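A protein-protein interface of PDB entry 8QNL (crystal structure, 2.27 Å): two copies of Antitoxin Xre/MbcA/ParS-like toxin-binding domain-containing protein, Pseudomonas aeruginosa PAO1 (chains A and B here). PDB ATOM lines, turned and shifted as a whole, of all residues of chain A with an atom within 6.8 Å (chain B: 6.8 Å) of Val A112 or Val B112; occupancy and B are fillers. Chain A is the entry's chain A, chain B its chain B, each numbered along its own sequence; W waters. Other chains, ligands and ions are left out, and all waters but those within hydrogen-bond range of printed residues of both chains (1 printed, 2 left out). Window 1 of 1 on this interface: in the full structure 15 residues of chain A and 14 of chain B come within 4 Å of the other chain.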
ATOM      1  N   GLY A  42      -5.383  17.075  -6.237  1.00  0.00           N
ATOM      2  CA  GLY A  42      -4.430  17.497  -7.248  1.00  0.00           C
ATOM      3  C   GLY A  42      -3.436  18.537  -6.782  1.00  0.00           C
ATOM      4  O   GLY A  42      -2.384  18.698  -7.410  1.00  0.00           O
ATOM      5  N   ILE A  43      -3.739  19.247  -5.696  1.00  0.00           N
ATOM      6  CA  ILE A  43      -2.829  20.272  -5.200  1.00  0.00           C
ATOM      7  C   ILE A  43      -1.748  19.653  -4.322  1.00  0.00           C
ATOM      8  O   ILE A  43      -0.554  19.916  -4.503  1.00  0.00           O
ATOM      9  CB  ILE A  43      -3.615  21.362  -4.446  1.00  0.00           C
ATOM     10  CG1 ILE A  43      -4.563  22.092  -5.399  1.00  0.00           C
ATOM     11  CG2 ILE A  43      -2.666  22.348  -3.777  1.00  0.00           C
ATOM     12  CD1 ILE A  43      -5.505  23.049  -4.701  1.00  0.00           C
ATOM     13  N   LYS A  64       6.545  15.443   1.969  1.00  0.00           N
ATOM     14  CA  LYS A  64       6.341  16.441   0.929  1.00  0.00           C
ATOM     15  C   LYS A  64       4.860  16.701   0.692  1.00  0.00           C
ATOM     16  O   LYS A  64       4.483  17.806   0.284  1.00  0.00           O
ATOM     17  CB  LYS A  64       7.020  15.989  -0.362  1.00  0.00           C
ATOM     18  CG  LYS A  64       7.312  17.124  -1.307  1.00  0.00           C
ATOM     19  CD  LYS A  64       8.320  18.086  -0.704  1.00  0.00           C
ATOM     20  CE  LYS A  64       9.659  17.422  -0.456  1.00  0.00           C
ATOM     21  NZ  LYS A  64      10.652  18.407   0.043  1.00  0.00           N
ATOM     22  N   GLU A  67       4.125  19.328   3.288  1.00  0.00           N
ATOM     23  CA  GLU A  67       4.662  20.634   2.906  1.00  0.00           C
ATOM     24  C   GLU A  67       3.754  21.334   1.908  1.00  0.00           C
ATOM     25  O   GLU A  67       3.486  22.534   2.033  1.00  0.00           O
ATOM     26  CB  GLU A  67       6.064  20.486   2.319  1.00  0.00           C
ATOM     27  CG  GLU A  67       7.169  20.325   3.351  1.00  0.00           C
ATOM     28  CD  GLU A  67       8.555  20.286   2.721  1.00  0.00           C
ATOM     29  OE1 GLU A  67       9.185  19.207   2.736  1.00  0.00           O
ATOM     30  OE2 GLU A  67       9.013  21.336   2.213  1.00  0.00           O
ATOM     31  N   LEU A  68       3.282  20.602   0.898  1.00  0.00           N
ATOM     32  CA  LEU A  68       2.353  21.191  -0.056  1.00  0.00           C
ATOM     33  C   LEU A  68       1.053  21.599   0.621  1.00  0.00           C
ATOM     34  O   LEU A  68       0.448  22.612   0.246  1.00  0.00           O
ATOM     35  CB  LEU A  68       2.092  20.213  -1.203  1.00  0.00           C
ATOM     36  CG  LEU A  68       3.319  19.856  -2.049  1.00  0.00           C
ATOM     37  CD1 LEU A  68       2.962  18.814  -3.095  1.00  0.00           C
ATOM     38  CD2 LEU A  68       3.907  21.093  -2.705  1.00  0.00           C
ATOM     39  N   LEU A  71       1.767  24.901   2.261  1.00  0.00           N
ATOM     40  CA  LEU A  71       1.696  25.980   1.280  1.00  0.00           C
ATOM     41  C   LEU A  71       0.252  26.303   0.923  1.00  0.00           C
ATOM     42  O   LEU A  71      -0.103  27.474   0.753  1.00  0.00           O
ATOM     43  CB  LEU A  71       2.482  25.606   0.021  1.00  0.00           C
ATOM     44  CG  LEU A  71       3.960  25.247   0.202  1.00  0.00           C
ATOM     45  CD1 LEU A  71       4.621  24.942  -1.142  1.00  0.00           C
ATOM     46  CD2 LEU A  71       4.703  26.359   0.933  1.00  0.00           C
ATOM     47  N   LEU A 108      -3.330  26.770 -11.648  1.00  0.00           N
ATOM     48  CA  LEU A 108      -1.885  26.830 -11.444  1.00  0.00           C
ATOM     49  C   LEU A 108      -1.455  26.008 -10.232  1.00  0.00           C
ATOM     50  O   LEU A 108      -0.428  25.321 -10.277  1.00  0.00           O
ATOM     51  CB  LEU A 108      -1.440  28.283 -11.290  1.00  0.00           C
ATOM     52  CG  LEU A 108      -1.689  29.194 -12.492  1.00  0.00           C
ATOM     53  CD1 LEU A 108      -1.354  30.628 -12.129  1.00  0.00           C
ATOM     54  CD2 LEU A 108      -0.879  28.736 -13.704  1.00  0.00           C
ATOM     55  N   MET A 109      -2.231  26.055  -9.146  1.00  0.00           N
ATOM     56  CA  MET A 109      -1.897  25.303  -7.940  1.00  0.00           C
ATOM     57  C   MET A 109      -1.941  23.794  -8.141  1.00  0.00           C
ATOM     58  O   MET A 109      -1.462  23.061  -7.269  1.00  0.00           O
ATOM     59  CB  MET A 109      -2.839  25.706  -6.807  1.00  0.00           C
ATOM     60  CG  MET A 109      -2.665  27.163  -6.401  1.00  0.00           C
ATOM     61  SD  MET A 109      -4.094  27.873  -5.570  1.00  0.00           S
ATOM     62  CE  MET A 109      -4.152  26.853  -4.112  1.00  0.00           C
ATOM     63  N   GLY A 110      -2.499  23.312  -9.254  1.00  0.00           N
ATOM     64  CA  GLY A 110      -2.435  21.893  -9.552  1.00  0.00           C
ATOM     65  C   GLY A 110      -1.027  21.374  -9.765  1.00  0.00           C
ATOM     66  O   GLY A 110      -0.793  20.167  -9.631  1.00  0.00           O
ATOM     67  N   GLN A 111      -0.085  22.254 -10.092  1.00  0.00           N
ATOM     68  CA  GLN A 111       1.318  21.895 -10.213  1.00  0.00           C
ATOM     69  C   GLN A 111       2.132  22.586  -9.127  1.00  0.00           C
ATOM     70  O   GLN A 111       1.750  23.635  -8.602  1.00  0.00           O
ATOM     71  CB  GLN A 111       1.877  22.264 -11.595  1.00  0.00           C
ATOM     72  CG  GLN A 111       1.437  21.342 -12.719  1.00  0.00           C
ATOM     73  CD  GLN A 111       0.026  21.628 -13.189  1.00  0.00           C
ATOM     74  OE1 GLN A 111      -0.463  22.754 -13.074  1.00  0.00           O
ATOM     75  NE2 GLN A 111      -0.640  20.605 -13.720  1.00  0.00           N
ATOM     76  N   VAL A 112       3.275  21.977  -8.806  1.00  0.00           N
ATOM     77  CA  VAL A 112       4.116  22.471  -7.718  1.00  0.00           C
ATOM     78  C   VAL A 112       4.588  23.892  -8.004  1.00  0.00           C
ATOM     79  O   VAL A 112       4.451  24.790  -7.165  1.00  0.00           O
ATOM     80  CB  VAL A 112       5.305  21.523  -7.486  1.00  0.00           C
ATOM     81  CG1 VAL A 112       6.306  22.155  -6.536  1.00  0.00           C
ATOM     82  CG2 VAL A 112       4.816  20.189  -6.946  1.00  0.00           C
ATOM     83  N   GLN A 113       5.158  24.117  -9.192  1.00  0.00           N
ATOM     84  CA  GLN A 113       5.691  25.440  -9.513  1.00  0.00           C
ATOM     85  C   GLN A 113       4.592  26.492  -9.587  1.00  0.00           C
ATOM     86  O   GLN A 113       4.831  27.665  -9.265  1.00  0.00           O
ATOM     87  CB  GLN A 113       6.473  25.390 -10.825  1.00  0.00           C
ATOM     88  CG  GLN A 113       7.312  26.625 -11.088  1.00  0.00           C
ATOM     89  CD  GLN A 113       8.306  26.425 -12.214  1.00  0.00           C
ATOM     90  OE1 GLN A 113       8.218  25.457 -12.971  1.00  0.00           O
ATOM     91  NE2 GLN A 113       9.266  27.335 -12.325  1.00  0.00           N
ATOM     92  N   GLY A 114       3.387  26.102 -10.005  1.00  0.00           N
ATOM     93  CA  GLY A 114       2.277  27.037  -9.998  1.00  0.00           C
ATOM     94  C   GLY A 114       1.784  27.350  -8.600  1.00  0.00           C
ATOM     95  O   GLY A 114       1.417  28.492  -8.310  1.00  0.00           O
ATOM     96  N   LEU A 115       1.777  26.351  -7.713  1.00  0.00           N
ATOM     97  CA  LEU A 115       1.400  26.595  -6.325  1.00  0.00           C
ATOM     98  C   LEU A 115       2.341  27.592  -5.662  1.00  0.00           C
ATOM     99  O   LEU A 115       1.894  28.501  -4.955  1.00  0.00           O
ATOM    100  CB  LEU A 115       1.384  25.281  -5.549  1.00  0.00           C
ATOM    101  CG  LEU A 115       1.108  25.388  -4.055  1.00  0.00           C
ATOM    102  CD1 LEU A 115      -0.250  26.028  -3.802  1.00  0.00           C
ATOM    103  CD2 LEU A 115       1.185  24.010  -3.421  1.00  0.00           C
ATOM    104  N   VAL A 116       3.650  27.438  -5.880  1.00  0.00           N
ATOM    105  CA  VAL A 116       4.604  28.392  -5.324  1.00  0.00           C
ATOM    106  C   VAL A 116       4.416  29.760  -5.965  1.00  0.00           C
ATOM    107  O   VAL A 116       4.501  30.795  -5.292  1.00  0.00           O
ATOM    108  CB  VAL A 116       6.043  27.869  -5.499  1.00  0.00           C
ATOM    109  CG1 VAL A 116       7.052  28.871  -4.958  1.00  0.00           C
ATOM    110  CG2 VAL A 116       6.197  26.531  -4.796  1.00  0.00           C
ATOM    111  N   HIS A 117       4.137  29.786  -7.269  1.00  0.00           N
ATOM    112  CA  HIS A 117       3.917  31.051  -7.962  1.00  0.00           C
ATOM    113  C   HIS A 117       2.730  31.805  -7.371  1.00  0.00           C
ATOM    114  O   HIS A 117       2.817  33.012  -7.115  1.00  0.00           O
ATOM    115  CB  HIS A 117       3.710  30.783  -9.454  1.00  0.00           C
ATOM    116  CG  HIS A 117       3.654  32.017 -10.298  1.00  0.00           C
ATOM    117  ND1 HIS A 117       2.854  32.114 -11.417  1.00  0.00           N
ATOM    118  CD2 HIS A 117       4.310  33.199 -10.202  1.00  0.00           C
ATOM    119  CE1 HIS A 117       3.012  33.304 -11.967  1.00  0.00           C
ATOM    120  NE2 HIS A 117       3.890  33.981 -11.250  1.00  0.00           N
ATOM    121  N   ILE B  43      14.930  16.245  -1.220  1.00  0.00           N
ATOM    122  CA  ILE B  43      14.569  17.269  -2.196  1.00  0.00           C
ATOM    123  C   ILE B  43      13.309  16.875  -2.952  1.00  0.00           C
ATOM    124  O   ILE B  43      12.410  17.700  -3.147  1.00  0.00           O
ATOM    125  CB  ILE B  43      15.748  17.530  -3.159  1.00  0.00           C
ATOM    126  CG1 ILE B  43      16.923  18.160  -2.404  1.00  0.00           C
ATOM    127  CG2 ILE B  43      15.314  18.436  -4.300  1.00  0.00           C
ATOM    128  CD1 ILE B  43      18.130  18.422  -3.277  1.00  0.00           C
ATOM    129  N   SER B  63       3.451  12.744 -10.883  1.00  0.00           N
ATOM    130  CA  SER B  63       3.490  12.784  -9.428  1.00  0.00           C
ATOM    131  C   SER B  63       4.155  14.063  -8.936  1.00  0.00           C
ATOM    132  O   SER B  63       4.890  14.733  -9.665  1.00  0.00           O
ATOM    133  CB  SER B  63       4.237  11.567  -8.876  1.00  0.00           C
ATOM    134  OG  SER B  63       5.571  11.541  -9.353  1.00  0.00           O
ATOM    135  N   LYS B  64       3.892  14.393  -7.669  1.00  0.00           N
ATOM    136  CA  LYS B  64       4.572  15.530  -7.058  1.00  0.00           C
ATOM    137  C   LYS B  64       6.066  15.270  -6.948  1.00  0.00           C
ATOM    138  O   LYS B  64       6.879  16.188  -7.108  1.00  0.00           O
ATOM    139  CB  LYS B  64       3.969  15.835  -5.687  1.00  0.00           C
ATOM    140  CG  LYS B  64       2.509  16.244  -5.748  1.00  0.00           C
ATOM    141  CD  LYS B  64       2.318  17.469  -6.630  1.00  0.00           C
ATOM    142  CE  LYS B  64       0.847  17.843  -6.760  1.00  0.00           C
ATOM    143  NZ  LYS B  64       0.643  18.964  -7.724  1.00  0.00           N
ATOM    144  N   THR B  65       6.448  14.020  -6.680  1.00  0.00           N
ATOM    145  CA  THR B  65       7.858  13.656  -6.719  1.00  0.00           C
ATOM    146  C   THR B  65       8.432  13.860  -8.116  1.00  0.00           C
ATOM    147  O   THR B  65       9.587  14.278  -8.267  1.00  0.00           O
ATOM    148  CB  THR B  65       8.035  12.207  -6.263  1.00  0.00           C
ATOM    149  OG1 THR B  65       7.445  12.039  -4.968  1.00  0.00           O
ATOM    150  CG2 THR B  65       9.509  11.843  -6.187  1.00  0.00           C
ATOM    151  N   GLU B  67       7.297  16.113 -10.354  1.00  0.00           N
ATOM    152  CA  GLU B  67       7.390  17.557 -10.549  1.00  0.00           C
ATOM    153  C   GLU B  67       8.620  18.132  -9.855  1.00  0.00           C
ATOM    154  O   GLU B  67       9.298  19.009 -10.404  1.00  0.00           O
ATOM    155  CB  GLU B  67       6.121  18.236 -10.036  1.00  0.00           C
ATOM    156  CG  GLU B  67       4.846  17.767 -10.711  1.00  0.00           C
ATOM    157  CD  GLU B  67       3.636  18.575 -10.284  1.00  0.00           C
ATOM    158  OE1 GLU B  67       3.782  19.799 -10.086  1.00  0.00           O
ATOM    159  OE2 GLU B  67       2.543  17.986 -10.143  1.00  0.00           O
ATOM    160  N   LEU B  68       8.921  17.656  -8.645  1.00  0.00           N
ATOM    161  CA  LEU B  68      10.106  18.134  -7.939  1.00  0.00           C
ATOM    162  C   LEU B  68      11.379  17.597  -8.573  1.00  0.00           C
ATOM    163  O   LEU B  68      12.399  18.293  -8.615  1.00  0.00           O
ATOM    164  CB  LEU B  68      10.043  17.731  -6.471  1.00  0.00           C
ATOM    165  CG  LEU B  68       8.886  18.321  -5.675  1.00  0.00           C
ATOM    166  CD1 LEU B  68       8.760  17.563  -4.384  1.00  0.00           C
ATOM    167  CD2 LEU B  68       9.100  19.808  -5.419  1.00  0.00           C
ATOM    168  N   LEU B  71      12.046  19.816 -11.367  1.00  0.00           N
ATOM    169  CA  LEU B  71      12.614  21.071 -10.887  1.00  0.00           C
ATOM    170  C   LEU B  71      14.091  20.911 -10.548  1.00  0.00           C
ATOM    171  O   LEU B  71      14.897  21.811 -10.811  1.00  0.00           O
ATOM    172  CB  LEU B  71      11.830  21.577  -9.673  1.00  0.00           C
ATOM    173  CG  LEU B  71      10.455  22.182  -9.977  1.00  0.00           C
ATOM    174  CD1 LEU B  71       9.760  22.635  -8.700  1.00  0.00           C
ATOM    175  CD2 LEU B  71      10.588  23.342 -10.953  1.00  0.00           C
ATOM    176  N   LEU B 108      18.588  25.107   0.878  1.00  0.00           N
ATOM    177  CA  LEU B 108      17.354  25.750   0.437  1.00  0.00           C
ATOM    178  C   LEU B 108      16.491  24.794  -0.374  1.00  0.00           C
ATOM    179  O   LEU B 108      15.262  24.785  -0.235  1.00  0.00           O
ATOM    180  CB  LEU B 108      17.678  26.999  -0.382  1.00  0.00           C
ATOM    181  CG  LEU B 108      18.067  28.258   0.393  1.00  0.00           C
ATOM    182  CD1 LEU B 108      18.672  29.294  -0.537  1.00  0.00           C
ATOM    183  CD2 LEU B 108      16.849  28.823   1.100  1.00  0.00           C
ATOM    184  N   MET B 109      17.115  23.980  -1.227  1.00  0.00           N
ATOM    185  CA  MET B 109      16.378  23.051  -2.074  1.00  0.00           C
ATOM    186  C   MET B 109      15.711  21.933  -1.287  1.00  0.00           C
ATOM    187  O   MET B 109      14.920  21.182  -1.866  1.00  0.00           O
ATOM    188  CB  MET B 109      17.314  22.466  -3.132  1.00  0.00           C
ATOM    189  CG  MET B 109      17.732  23.476  -4.186  1.00  0.00           C
ATOM    190  SD  MET B 109      19.349  23.135  -4.919  1.00  0.00           S
ATOM    191  CE  MET B 109      19.108  21.463  -5.503  1.00  0.00           C
ATOM    192  N   GLY B 110      16.010  21.805   0.008  1.00  0.00           N
ATOM    193  CA  GLY B 110      15.342  20.817   0.833  1.00  0.00           C
ATOM    194  C   GLY B 110      13.870  21.093   1.053  1.00  0.00           C
ATOM    195  O   GLY B 110      13.131  20.180   1.438  1.00  0.00           O
ATOM    196  N   GLN B 111      13.425  22.327   0.822  1.00  0.00           N
ATOM    197  CA  GLN B 111      12.018  22.678   0.905  1.00  0.00           C
ATOM    198  C   GLN B 111      11.509  23.094  -0.470  1.00  0.00           C
ATOM    199  O   GLN B 111      12.282  23.467  -1.359  1.00  0.00           O
ATOM    200  CB  GLN B 111      11.775  23.803   1.921  1.00  0.00           C
ATOM    201  CG  GLN B 111      12.303  25.156   1.491  1.00  0.00           C
ATOM    202  CD  GLN B 111      11.869  26.267   2.425  1.00  0.00           C
ATOM    203  OE1 GLN B 111      11.327  27.286   1.988  1.00  0.00           O
ATOM    204  NE2 GLN B 111      12.104  26.079   3.721  1.00  0.00           N
ATOM    205  N   VAL B 112      10.185  23.031  -0.631  1.00  0.00           N
ATOM    206  CA  VAL B 112       9.575  23.261  -1.939  1.00  0.00           C
ATOM    207  C   VAL B 112       9.837  24.682  -2.413  1.00  0.00           C
ATOM    208  O   VAL B 112      10.294  24.907  -3.541  1.00  0.00           O
ATOM    209  CB  VAL B 112       8.069  22.960  -1.886  1.00  0.00           C
ATOM    210  CG1 VAL B 112       7.399  23.399  -3.182  1.00  0.00           C
ATOM    211  CG2 VAL B 112       7.843  21.488  -1.645  1.00  0.00           C
ATOM    212  N   GLN B 113       9.540  25.663  -1.562  1.00  0.00           N
ATOM    213  CA  GLN B 113       9.687  27.054  -1.969  1.00  0.00           C
ATOM    214  C   GLN B 113      11.150  27.425  -2.181  1.00  0.00           C
ATOM    215  O   GLN B 113      11.461  28.241  -3.056  1.00  0.00           O
ATOM    216  CB  GLN B 113       9.030  27.967  -0.932  1.00  0.00           C
ATOM    217  CG  GLN B 113       8.809  29.382  -1.414  1.00  0.00           C
ATOM    218  CD  GLN B 113       7.860  30.167  -0.529  1.00  0.00           C
ATOM    219  OE1 GLN B 113       7.316  29.641   0.445  1.00  0.00           O
ATOM    220  NE2 GLN B 113       7.656  31.434  -0.866  1.00  0.00           N
ATOM    221  N   GLY B 114      12.061  26.837  -1.404  1.00  0.00           N
ATOM    222  CA  GLY B 114      13.474  27.075  -1.635  1.00  0.00           C
ATOM    223  C   GLY B 114      13.981  26.434  -2.910  1.00  0.00           C
ATOM    224  O   GLY B 114      14.870  26.979  -3.572  1.00  0.00           O
ATOM    225  N   LEU B 115      13.425  25.277  -3.276  1.00  0.00           N
ATOM    226  CA  LEU B 115      13.807  24.641  -4.533  1.00  0.00           C
ATOM    227  C   LEU B 115      13.443  25.521  -5.721  1.00  0.00           C
ATOM    228  O   LEU B 115      14.239  25.679  -6.654  1.00  0.00           O
ATOM    229  CB  LEU B 115      13.144  23.270  -4.649  1.00  0.00           C
ATOM    230  CG  LEU B 115      13.326  22.529  -5.977  1.00  0.00           C
ATOM    231  CD1 LEU B 115      14.802  22.327  -6.306  1.00  0.00           C
ATOM    232  CD2 LEU B 115      12.594  21.195  -5.944  1.00  0.00           C
ATOM    233  N   VAL B 116      12.247  26.114  -5.698  1.00  0.00           N
ATOM    234  CA  VAL B 116      11.856  27.040  -6.754  1.00  0.00           C
ATOM    235  C   VAL B 116      12.723  28.293  -6.715  1.00  0.00           C
ATOM    236  O   VAL B 116      13.129  28.815  -7.761  1.00  0.00           O
ATOM    237  CB  VAL B 116      10.358  27.380  -6.635  1.00  0.00           C
ATOM    238  CG1 VAL B 116       9.976  28.478  -7.616  1.00  0.00           C
ATOM    239  CG2 VAL B 116       9.514  26.136  -6.875  1.00  0.00           C
ATOM    240  N   HIS B 117      13.038  28.781  -5.515  1.00  0.00           N
ATOM    241  CA  HIS B 117      13.806  30.017  -5.400  1.00  0.00           C
ATOM    242  C   HIS B 117      15.212  29.858  -5.968  1.00  0.00           C
ATOM    243  O   HIS B 117      15.736  30.777  -6.610  1.00  0.00           O
ATOM    244  CB  HIS B 117      13.867  30.465  -3.940  1.00  0.00           C
ATOM    245  CG  HIS B 117      14.675  31.706  -3.726  1.00  0.00           C
ATOM    246  ND1 HIS B 117      14.572  32.809  -4.546  1.00  0.00           N
ATOM    247  CD2 HIS B 117      15.603  32.017  -2.791  1.00  0.00           C
ATOM    248  CE1 HIS B 117      15.400  33.747  -4.124  1.00  0.00           C
ATOM    249  NE2 HIS B 117      16.037  33.293  -3.060  1.00  0.00           N
HETATM  250  O   HOH W   1       5.675  22.038 -11.170  1.00  0.00           O
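OE1 of Glu A67 lies within salt-bridge range of NZ of Lys A64 (3.2 Å). NZ of Lys B64 lies within salt-bridge range of OE2 of Glu B67, 3.2 Å away. N of Gly B114 lies close to OE1 of Gln B111 (3.5 Å).
Of the 17 printed residues of chain B, 10 touch a printed residue of chain A. Hydrophobic or aromatic side chains of chain B that line the printed part of chain A: Leu B68, Leu B71, Val B112 and Val B116. Along chain B the printed residues that touch a printed residue of chain A span positions 43 to 116. Among the printed residues, no Asp or Glu carboxylate lies within 4 Å of a Lys or Arg side-chain nitrogen of the other chain.
Lys A64 touches Leu B68, and with the chains exchanged Leu A68 touches Lys B64. Lys A64 touches Gly B110, and with the chains exchanged Gly A110 touches Lys B64. Glu A67 touches Gln B111, and with the chains exchanged Gln A111 touches Glu B67. Gln A113 touches Leu B71, but with the chains exchanged Leu A71 does not touch Gln B113 (4.2 Å). Of the 21 pairs that touch across the chains among the printed residues, 14 have their exchanged pair printed and touching as well.
Among the printed residues, pairs that only touch across the chains: Gln A111 with Glu B67 (3.2 Å), Ile A43 with Lys B64 (3.4 Å), Lys A64 with Leu B68 (3.4 Å), Glu A67 with Val B112 (3.5 Å), Glu A67 with Gln B111 (3.5 Å), Lys A64 with Val B112 (3.6 Å), Val A112 with Lys B64 (3.7 Å), Lys A64 with Ile B43 (3.7 Å), Leu A68 with Lys B64 (3.7 Å), Val A116 with Val B112 (3.7 Å), Val A112 with Val B112 (3.7 Å), Gln A113 with Leu B71 (3.8 Å), Leu A71 with Val B112 (3.8 Å), Val A112 with Leu B68 (3.8 Å), Gln A111 with Lys B64 (3.9 Å), Val A116 with Val B116 (3.9 Å) and Val A116 with Gln B113 (3.99 Å).
The side-chain amino group (NZ) of Lys B64 is in hydrogen-bond range of the backbone carbonyl oxygen (O) of Gly A42 (3.1 Å). NZ of Lys A64 is in hydrogen-bond range of O of Gly B110 (3.4 Å). The backbone carbonyl oxygen of Gly A110 is in hydrogen-bond range of the side-chain amino group of Lys B64 (2.7 Å). N of Val A112 is in hydrogen-bond range of OE1 of Glu B67, at 2.6 Å.
Water W1 lies within hydrogen-bond range of N of Gln A113, OE1 of Glu B67 and N of Val A112.
Of the printed residues of chain B, Val A112 touches Lys B64 (3.7 Å), Glu B67 (2.6 Å), Leu B68 (3.8 Å) and Val B112 (3.7 Å). Of the printed residues of chain A, Val B112 touches Lys A64 (3.6 Å), Glu A67 (3.5 Å), Leu A71 (3.8 Å), Val A112 (3.7 Å) and Val A116 (3.7 Å). Of the printed residues of chain B, Lys A64 touches Ile B43 (3.7 Å), Leu B68 (3.4 Å), Gly B110 (3.4 Å) and Val B112 (3.6 Å). Of the printed residues of chain A, Val B116 touches Val A116 (3.9 Å). Gly B114 touches none of the printed residues of chain A.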
